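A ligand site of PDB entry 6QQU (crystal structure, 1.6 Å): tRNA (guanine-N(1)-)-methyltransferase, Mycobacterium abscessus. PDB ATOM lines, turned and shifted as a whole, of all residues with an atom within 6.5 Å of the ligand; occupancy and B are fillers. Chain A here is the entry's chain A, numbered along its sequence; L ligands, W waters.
N2 of the ligand is in hydrogen-bond range of O of Tyr 138 (2.6 Å). The backbone carbonyl oxygen of Gly 136 is in hydrogen-bond range of a nitrogen (N1) of the ligand, at 2.9 Å. N3 of the ligand lies within hydrogen-bond range of N of Leu 140 (3.0 Å). A nitrogen (N1) of the ligand sits at hydrogen-bond distance from the side-chain hydroxyl (OG) of Ser 134 (3.0 Å). N of Thr 86 is in hydrogen-bond range of N5 of the ligand (3.3 Å).
The backbone carbonyl oxygen (O) of Ile 135 sits at hydrogen-bond distance from the side-chain hydroxyl (OH) of Tyr 138, at 3.2 Å. OG of Ser 134 sits at hydrogen-bond distance from O of Gly 136, 3.0 Å away. The backbone carbonyl oxygen (O) of Val 133 lies within hydrogen-bond range of the backbone NH (N) of Thr 86 (2.9 Å). The backbone NH (N) of Val 133 lies within hydrogen-bond range of the backbone carbonyl oxygen (O) of Val 84. The side-chain hydroxyl of Thr 86 lies close to the backbone NH of Ala 88, 3.0 Å away. O of Gly 111 is in hydrogen-bond range of N of Gly 143, at 2.9 Å. The side-chain carboxylate of Glu 144 is in salt-bridge range of the guanidinium group of Arg 112, 2.8 Å away.
O of Val 133 sits close to N5 of the ligand (3.3 Å). Merely in contact with the ligand: Pro 85 (3.2 Å), Tyr 113 (3.3 Å), Gly 111 (3.4 Å), Pro 87 (3.4 Å), Gly 143 (3.5 Å), Ala 146 (3.5 Å), Gly 142 (3.5 Å), Ile 135 (3.6 Å), Asn 141 (3.6 Å), Val 139 (3.7 Å) and Arg 112 (3.7 Å). Hydrophobic or aromatic side chains within 4 Å of the ligand: Pro 85, Pro 87, Ile 135, Tyr 138, Leu 140 and Ala 146. 17 residues have an atom within 4 Å of the ligand: Pro 85, Thr 86, Pro 87, Gly 111, Arg 112, Tyr 113, Val 133, Ser 134, Ile 135, Gly 136, Tyr 138, Val 139, Leu 140, Asn 141, Gly 142, Gly 143 and Ala 146. Along chain A the residues within 4 Å of the ligand span positions 85 to 146.
Water W1 lies within hydrogen-bond range of the backbone carbonyl oxygen of Leu 140 and a nitrogen (N4) of the ligand.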
ATOM      1  N   VAL A  84     -24.364  -2.633 -12.636  1.00  0.00           N
ATOM      2  CA  VAL A  84     -25.624  -1.908 -12.751  1.00  0.00           C
ATOM      3  C   VAL A  84     -25.817  -0.988 -11.551  1.00  0.00           C
ATOM      4  O   VAL A  84     -26.186  -1.437 -10.447  1.00  0.00           O
ATOM      5  CB  VAL A  84     -26.825  -2.878 -12.848  1.00  0.00           C
ATOM      6  CG1 VAL A  84     -28.097  -2.090 -13.054  1.00  0.00           C
ATOM      7  CG2 VAL A  84     -26.613  -3.887 -13.981  1.00  0.00           C
ATOM      8  N   PRO A  85     -25.509   0.306 -11.719  1.00  0.00           N
ATOM      9  CA  PRO A  85     -25.767   1.247 -10.627  1.00  0.00           C
ATOM     10  C   PRO A  85     -27.259   1.315 -10.292  1.00  0.00           C
ATOM     11  O   PRO A  85     -28.106   1.351 -11.194  1.00  0.00           O
ATOM     12  CB  PRO A  85     -25.262   2.583 -11.191  1.00  0.00           C
ATOM     13  CG  PRO A  85     -24.199   2.192 -12.185  1.00  0.00           C
ATOM     14  CD  PRO A  85     -24.756   0.929 -12.827  1.00  0.00           C
ATOM     15  N   THR A  86     -27.557   1.325  -9.001  1.00  0.00           N
ATOM     16  CA  THR A  86     -28.940   1.462  -8.545  1.00  0.00           C
ATOM     17  C   THR A  86     -28.925   1.843  -7.083  1.00  0.00           C
ATOM     18  O   THR A  86     -28.065   1.379  -6.339  1.00  0.00           O
ATOM     19  CB  THR A  86     -29.742   0.157  -8.749  1.00  0.00           C
ATOM     20  OG1 THR A  86     -30.918   0.167  -7.931  1.00  0.00           O
ATOM     21  CG2 THR A  86     -28.886  -1.059  -8.412  1.00  0.00           C
ATOM     22  N   PRO A  87     -29.863   2.710  -6.669  1.00  0.00           N
ATOM     23  CA  PRO A  87     -29.908   3.086  -5.255  1.00  0.00           C
ATOM     24  C   PRO A  87     -30.247   1.889  -4.374  1.00  0.00           C
ATOM     25  O   PRO A  87     -29.971   1.936  -3.170  1.00  0.00           O
ATOM     26  CB  PRO A  87     -31.010   4.163  -5.208  1.00  0.00           C
ATOM     27  CG  PRO A  87     -31.785   4.015  -6.446  1.00  0.00           C
ATOM     28  CD  PRO A  87     -30.906   3.353  -7.468  1.00  0.00           C
ATOM     29  N   ALA A  88     -30.784   0.828  -4.961  1.00  0.00           N
ATOM     30  CA  ALA A  88     -31.103  -0.395  -4.229  1.00  0.00           C
ATOM     31  C   ALA A  88     -29.990  -1.452  -4.313  1.00  0.00           C
ATOM     32  O   ALA A  88     -30.222  -2.614  -3.999  1.00  0.00           O
ATOM     33  CB  ALA A  88     -32.423  -0.977  -4.735  1.00  0.00           C
ATOM     34  N   ALA A 109     -24.129  -0.512 -17.031  1.00  0.00           N
ATOM     35  CA  ALA A 109     -25.451  -0.227 -17.579  1.00  0.00           C
ATOM     36  C   ALA A 109     -26.108   0.891 -16.781  1.00  0.00           C
ATOM     37  O   ALA A 109     -26.575   0.683 -15.649  1.00  0.00           O
ATOM     38  CB  ALA A 109     -26.328  -1.475 -17.556  1.00  0.00           C
ATOM     39  N   CYS A 110     -26.154   2.075 -17.383  1.00  0.00           N
ATOM     40  CA  CYS A 110     -26.689   3.251 -16.711  1.00  0.00           C
ATOM     41  C   CYS A 110     -28.177   3.421 -16.927  1.00  0.00           C
ATOM     42  O   CYS A 110     -28.620   3.703 -18.053  1.00  0.00           O
ATOM     43  CB  CYS A 110     -25.993   4.506 -17.187  1.00  0.00           C
ATOM     44  SG  CYS A 110     -24.245   4.567 -16.829  1.00  0.00           S
ATOM     45  N   GLY A 111     -28.955   3.294 -15.858  1.00  0.00           N
ATOM     46  CA  GLY A 111     -30.377   3.523 -15.969  1.00  0.00           C
ATOM     47  C   GLY A 111     -30.787   4.980 -15.811  1.00  0.00           C
ATOM     48  O   GLY A 111     -29.996   5.832 -15.403  1.00  0.00           O
ATOM     49  N   ARG A 112     -32.053   5.231 -16.112  1.00  0.00           N
ATOM     50  CA  ARG A 112     -32.701   6.514 -15.904  1.00  0.00           C
ATOM     51  C   ARG A 112     -34.142   6.223 -15.499  1.00  0.00           C
ATOM     52  O   ARG A 112     -34.510   5.051 -15.321  1.00  0.00           O
ATOM     53  CB  ARG A 112     -32.615   7.399 -17.164  1.00  0.00           C
ATOM     54  CG  ARG A 112     -31.258   8.094 -17.338  1.00  0.00           C
ATOM     55  CD  ARG A 112     -31.259   9.453 -16.617  1.00  0.00           C
ATOM     56  NE  ARG A 112     -29.908   9.890 -16.268  1.00  0.00           N
ATOM     57  CZ  ARG A 112     -29.603  11.109 -15.842  1.00  0.00           C
ATOM     58  NH1 ARG A 112     -30.540  12.052 -15.732  1.00  0.00           N
ATOM     59  NH2 ARG A 112     -28.327  11.391 -15.539  1.00  0.00           N
ATOM     60  N   TYR A 113     -34.957   7.262 -15.359  1.00  0.00           N
ATOM     61  CA  TYR A 113     -36.350   7.084 -14.937  1.00  0.00           C
ATOM     62  C   TYR A 113     -36.384   6.294 -13.623  1.00  0.00           C
ATOM     63  O   TYR A 113     -35.609   6.593 -12.711  1.00  0.00           O
ATOM     64  CB  TYR A 113     -37.156   6.361 -16.027  1.00  0.00           C
ATOM     65  CG  TYR A 113     -36.996   6.952 -17.414  1.00  0.00           C
ATOM     66  CD1 TYR A 113     -37.822   7.986 -17.856  1.00  0.00           C
ATOM     67  CD2 TYR A 113     -36.038   6.472 -18.294  1.00  0.00           C
ATOM     68  CE1 TYR A 113     -37.677   8.521 -19.121  1.00  0.00           C
ATOM     69  CE2 TYR A 113     -35.886   7.000 -19.558  1.00  0.00           C
ATOM     70  CZ  TYR A 113     -36.709   8.029 -19.967  1.00  0.00           C
ATOM     71  OH  TYR A 113     -36.563   8.548 -21.238  1.00  0.00           O
ATOM     72  N   GLU A 114     -37.241   5.284 -13.524  1.00  0.00           N
ATOM     73  CA  GLU A 114     -37.300   4.471 -12.307  1.00  0.00           C
ATOM     74  C   GLU A 114     -36.440   3.211 -12.385  1.00  0.00           C
ATOM     75  O   GLU A 114     -36.617   2.278 -11.597  1.00  0.00           O
ATOM     76  CB  GLU A 114     -38.746   4.091 -11.980  1.00  0.00           C
ATOM     77  CG  GLU A 114     -39.655   5.293 -11.748  1.00  0.00           C
ATOM     78  CD  GLU A 114     -39.045   6.292 -10.782  1.00  0.00           C
ATOM     79  OE1 GLU A 114     -38.740   7.424 -11.205  1.00  0.00           O
ATOM     80  OE2 GLU A 114     -38.869   5.931  -9.601  1.00  0.00           O
ATOM     81  N   GLY A 115     -35.506   3.192 -13.325  1.00  0.00           N
ATOM     82  CA  GLY A 115     -34.547   2.099 -13.423  1.00  0.00           C
ATOM     83  C   GLY A 115     -34.870   1.120 -14.533  1.00  0.00           C
ATOM     84  O   GLY A 115     -35.739   1.390 -15.356  1.00  0.00           O
ATOM     85  N   ILE A 116     -34.186  -0.022 -14.544  1.00  0.00           N
ATOM     86  CA  ILE A 116     -34.274  -0.995 -15.644  1.00  0.00           C
ATOM     87  C   ILE A 116     -35.115  -2.188 -15.232  1.00  0.00           C
ATOM     88  O   ILE A 116     -34.990  -2.680 -14.126  1.00  0.00           O
ATOM     89  CB  ILE A 116     -32.865  -1.461 -16.047  1.00  0.00           C
ATOM     90  CG1 ILE A 116     -31.959  -0.251 -16.321  1.00  0.00           C
ATOM     91  CG2 ILE A 116     -32.905  -2.417 -17.259  1.00  0.00           C
ATOM     92  CD1 ILE A 116     -30.526  -0.634 -16.572  1.00  0.00           C
ATOM     93  N   VAL A 133     -25.048  -2.338  -7.733  1.00  0.00           N
ATOM     94  CA  VAL A 133     -24.362  -1.638  -6.652  1.00  0.00           C
ATOM     95  C   VAL A 133     -24.807  -0.199  -6.518  1.00  0.00           C
ATOM     96  O   VAL A 133     -25.261   0.417  -7.480  1.00  0.00           O
ATOM     97  CB  VAL A 133     -22.823  -1.644  -6.839  1.00  0.00           C
ATOM     98  CG1 VAL A 133     -22.282  -3.049  -6.789  1.00  0.00           C
ATOM     99  CG2 VAL A 133     -22.420  -0.923  -8.148  1.00  0.00           C
ATOM    100  N   SER A 134     -24.680   0.332  -5.302  1.00  0.00           N
ATOM    101  CA  SER A 134     -24.976   1.739  -4.999  1.00  0.00           C
ATOM    102  C   SER A 134     -23.716   2.442  -4.484  1.00  0.00           C
ATOM    103  O   SER A 134     -23.020   1.892  -3.645  1.00  0.00           O
ATOM    104  CB  SER A 134     -26.060   1.858  -3.936  1.00  0.00           C
ATOM    105  OG  SER A 134     -26.178   3.198  -3.495  1.00  0.00           O
ATOM    106  N   ILE A 135     -23.464   3.660  -4.951  1.00  0.00           N
ATOM    107  CA  ILE A 135     -22.289   4.409  -4.477  1.00  0.00           C
ATOM    108  C   ILE A 135     -22.540   5.237  -3.216  1.00  0.00           C
ATOM    109  O   ILE A 135     -21.602   5.873  -2.711  1.00  0.00           O
ATOM    110  CB  ILE A 135     -21.749   5.352  -5.575  1.00  0.00           C
ATOM    111  CG1 ILE A 135     -22.806   6.378  -5.984  1.00  0.00           C
ATOM    112  CG2 ILE A 135     -21.277   4.551  -6.801  1.00  0.00           C
ATOM    113  CD1 ILE A 135     -22.196   7.636  -6.676  1.00  0.00           C
ATOM    114  N   GLY A 136     -23.765   5.247  -2.689  1.00  0.00           N
ATOM    115  CA  GLY A 136     -24.025   5.992  -1.456  1.00  0.00           C
ATOM    116  C   GLY A 136     -25.496   6.133  -1.133  1.00  0.00           C
ATOM    117  O   GLY A 136     -26.363   5.820  -1.954  1.00  0.00           O
ATOM    118  N   ASP A 137     -25.792   6.612   0.064  1.00  0.00           N
ATOM    119  CA  ASP A 137     -27.174   6.670   0.532  1.00  0.00           C
ATOM    120  C   ASP A 137     -27.840   8.002   0.216  1.00  0.00           C
ATOM    121  O   ASP A 137     -28.223   8.757   1.118  1.00  0.00           O
ATOM    122  CB  ASP A 137     -27.212   6.388   2.022  1.00  0.00           C
ATOM    123  CG  ASP A 137     -26.880   4.962   2.337  1.00  0.00           C
ATOM    124  OD1 ASP A 137     -27.070   4.101   1.438  1.00  0.00           O
ATOM    125  OD2 ASP A 137     -26.431   4.687   3.461  1.00  0.00           O
ATOM    126  N   TYR A 138     -27.979   8.269  -1.075  1.00  0.00           N
ATOM    127  CA  TYR A 138     -28.645   9.453  -1.598  1.00  0.00           C
ATOM    128  C   TYR A 138     -29.208   9.014  -2.927  1.00  0.00           C
ATOM    129  O   TYR A 138     -28.803   7.968  -3.454  1.00  0.00           O
ATOM    130  CB  TYR A 138     -27.665  10.635  -1.762  1.00  0.00           C
ATOM    131  CG  TYR A 138     -26.304  10.179  -2.218  1.00  0.00           C
ATOM    132  CD1 TYR A 138     -26.078   9.823  -3.552  1.00  0.00           C
ATOM    133  CD2 TYR A 138     -25.263  10.048  -1.307  1.00  0.00           C
ATOM    134  CE1 TYR A 138     -24.840   9.353  -3.958  1.00  0.00           C
ATOM    135  CE2 TYR A 138     -24.019   9.588  -1.705  1.00  0.00           C
ATOM    136  CZ  TYR A 138     -23.815   9.254  -3.034  1.00  0.00           C
ATOM    137  OH  TYR A 138     -22.591   8.788  -3.419  1.00  0.00           O
ATOM    138  N   VAL A 139     -30.119   9.803  -3.471  1.00  0.00           N
ATOM    139  CA  VAL A 139     -30.765   9.470  -4.733  1.00  0.00           C
ATOM    140  C   VAL A 139     -30.318  10.406  -5.846  1.00  0.00           C
ATOM    141  O   VAL A 139     -30.337  11.621  -5.697  1.00  0.00           O
ATOM    142  CB  VAL A 139     -32.282   9.527  -4.582  1.00  0.00           C
ATOM    143  CG1 VAL A 139     -32.958   9.099  -5.879  1.00  0.00           C
ATOM    144  CG2 VAL A 139     -32.730   8.632  -3.429  1.00  0.00           C
ATOM    145  N   LEU A 140     -29.920   9.793  -6.977  1.00  0.00           N
ATOM    146  CA  LEU A 140     -29.547  10.515  -8.192  1.00  0.00           C
ATOM    147  C   LEU A 140     -30.653  10.404  -9.228  1.00  0.00           C
ATOM    148  O   LEU A 140     -31.636   9.701  -9.015  1.00  0.00           O
ATOM    149  CB  LEU A 140     -28.232   9.944  -8.748  1.00  0.00           C
ATOM    150  CG  LEU A 140     -27.040   9.981  -7.798  1.00  0.00           C
ATOM    151  CD1 LEU A 140     -25.915   9.099  -8.309  1.00  0.00           C
ATOM    152  CD2 LEU A 140     -26.544  11.407  -7.648  1.00  0.00           C
ATOM    153  N   ASN A 141     -30.505  11.088 -10.360  1.00  0.00           N
ATOM    154  CA  ASN A 141     -31.475  11.002 -11.461  1.00  0.00           C
ATOM    155  C   ASN A 141     -31.283   9.767 -12.341  1.00  0.00           C
ATOM    156  O   ASN A 141     -32.180   9.369 -13.085  1.00  0.00           O
ATOM    157  CB  ASN A 141     -31.374  12.237 -12.354  1.00  0.00           C
ATOM    158  CG  ASN A 141     -31.872  13.479 -11.672  1.00  0.00           C
ATOM    159  OD1 ASN A 141     -32.892  13.458 -10.998  1.00  0.00           O
ATOM    160  ND2 ASN A 141     -31.143  14.584 -11.855  1.00  0.00           N
ATOM    161  N   GLY A 142     -30.095   9.182 -12.273  1.00  0.00           N
ATOM    162  CA  GLY A 142     -29.767   8.049 -13.105  1.00  0.00           C
ATOM    163  C   GLY A 142     -28.377   7.555 -12.770  1.00  0.00           C
ATOM    164  O   GLY A 142     -27.708   8.077 -11.866  1.00  0.00           O
ATOM    165  N   GLY A 143     -27.919   6.558 -13.512  1.00  0.00           N
ATOM    166  CA  GLY A 143     -26.676   5.880 -13.169  1.00  0.00           C
ATOM    167  C   GLY A 143     -25.378   6.529 -13.641  1.00  0.00           C
ATOM    168  O   GLY A 143     -24.302   6.073 -13.262  1.00  0.00           O
ATOM    169  N   GLU A 144     -25.461   7.563 -14.468  1.00  0.00           N
ATOM    170  CA  GLU A 144     -24.250   8.135 -15.070  1.00  0.00           C
ATOM    171  C   GLU A 144     -23.237   8.710 -14.059  1.00  0.00           C
ATOM    172  O   GLU A 144     -22.031   8.433 -14.165  1.00  0.00           O
ATOM    173  CB  GLU A 144     -24.633   9.206 -16.072  1.00  0.00           C
ATOM    174  CG  GLU A 144     -25.326   8.662 -17.355  1.00  0.00           C
ATOM    175  CD  GLU A 144     -26.802   8.333 -17.198  1.00  0.00           C
ATOM    176  OE1 GLU A 144     -27.407   8.648 -16.149  1.00  0.00           O
ATOM    177  OE2 GLU A 144     -27.363   7.757 -18.153  1.00  0.00           O
ATOM    178  N   ALA A 146     -22.927   7.831 -11.036  1.00  0.00           N
ATOM    179  CA  ALA A 146     -22.406   6.670 -10.326  1.00  0.00           C
ATOM    180  C   ALA A 146     -21.346   5.954 -11.163  1.00  0.00           C
ATOM    181  O   ALA A 146     -20.337   5.483 -10.631  1.00  0.00           O
ATOM    182  CB  ALA A 146     -23.533   5.712  -9.939  1.00  0.00           C
ATOM    183  N   ALA A 147     -21.558   5.898 -12.472  1.00  0.00           N
ATOM    184  CA  ALA A 147     -20.593   5.323 -13.377  1.00  0.00           C
ATOM    185  C   ALA A 147     -19.285   6.091 -13.331  1.00  0.00           C
ATOM    186  O   ALA A 147     -18.221   5.480 -13.334  1.00  0.00           O
ATOM    187  CB  ALA A 147     -21.141   5.287 -14.802  1.00  0.00           C
ATOM    188  N   ILE A 150     -17.535   5.117 -10.069  1.00  0.00           N
ATOM    189  CA  ILE A 150     -17.013   3.757 -10.135  1.00  0.00           C
ATOM    190  C   ILE A 150     -15.791   3.653 -11.042  1.00  0.00           C
ATOM    191  O   ILE A 150     -14.773   3.038 -10.677  1.00  0.00           O
ATOM    192  CB  ILE A 150     -18.117   2.772 -10.606  1.00  0.00           C
ATOM    193  CG1 ILE A 150     -19.158   2.600  -9.492  1.00  0.00           C
ATOM    194  CG2 ILE A 150     -17.487   1.419 -10.950  1.00  0.00           C
ATOM    195  CD1 ILE A 150     -20.502   2.056  -9.987  1.00  0.00           C
HETATM  196  C1  LIG L   1     -31.010   5.937 -10.577  1.00  0.00           C
HETATM  197  C2  LIG L   1     -31.451   4.876 -12.502  1.00  0.00           C
HETATM  198  C3  LIG L   1     -27.326   5.505  -7.157  1.00  0.00           C
HETATM  199  N1  LIG L   1     -26.263   5.901  -4.899  1.00  0.00           N
HETATM  200  C4  LIG L   1     -27.256   6.130  -5.924  1.00  0.00           C
HETATM  201  N2  LIG L   1     -28.282   7.017  -5.847  1.00  0.00           N
HETATM  202  N3  LIG L   1     -28.986   6.931  -7.001  1.00  0.00           N
HETATM  203  C5  LIG L   1     -28.409   6.063  -7.826  1.00  0.00           C
HETATM  204  C6  LIG L   1     -29.066   5.716  -9.157  1.00  0.00           C
HETATM  205  C7  LIG L   1     -28.537   4.716 -10.014  1.00  0.00           C
HETATM  206  C8  LIG L   1     -29.239   4.371 -11.167  1.00  0.00           C
HETATM  207  C9  LIG L   1     -30.487   4.994 -11.441  1.00  0.00           C
HETATM  208  N4  LIG L   1     -32.214   6.384 -11.073  1.00  0.00           N
HETATM  209  C10 LIG L   1     -32.479   5.761 -12.225  1.00  0.00           C
HETATM  210  C11 LIG L   1     -30.300   6.301  -9.389  1.00  0.00           C
HETATM  211  C12 LIG L   1     -26.311   4.469  -7.598  1.00  0.00           C
HETATM  212  N5  LIG L   1     -25.514   3.699  -7.877  1.00  0.00           N
HETATM  213  O   HOH W   1     -33.908   8.239  -9.601  1.00  0.00           O
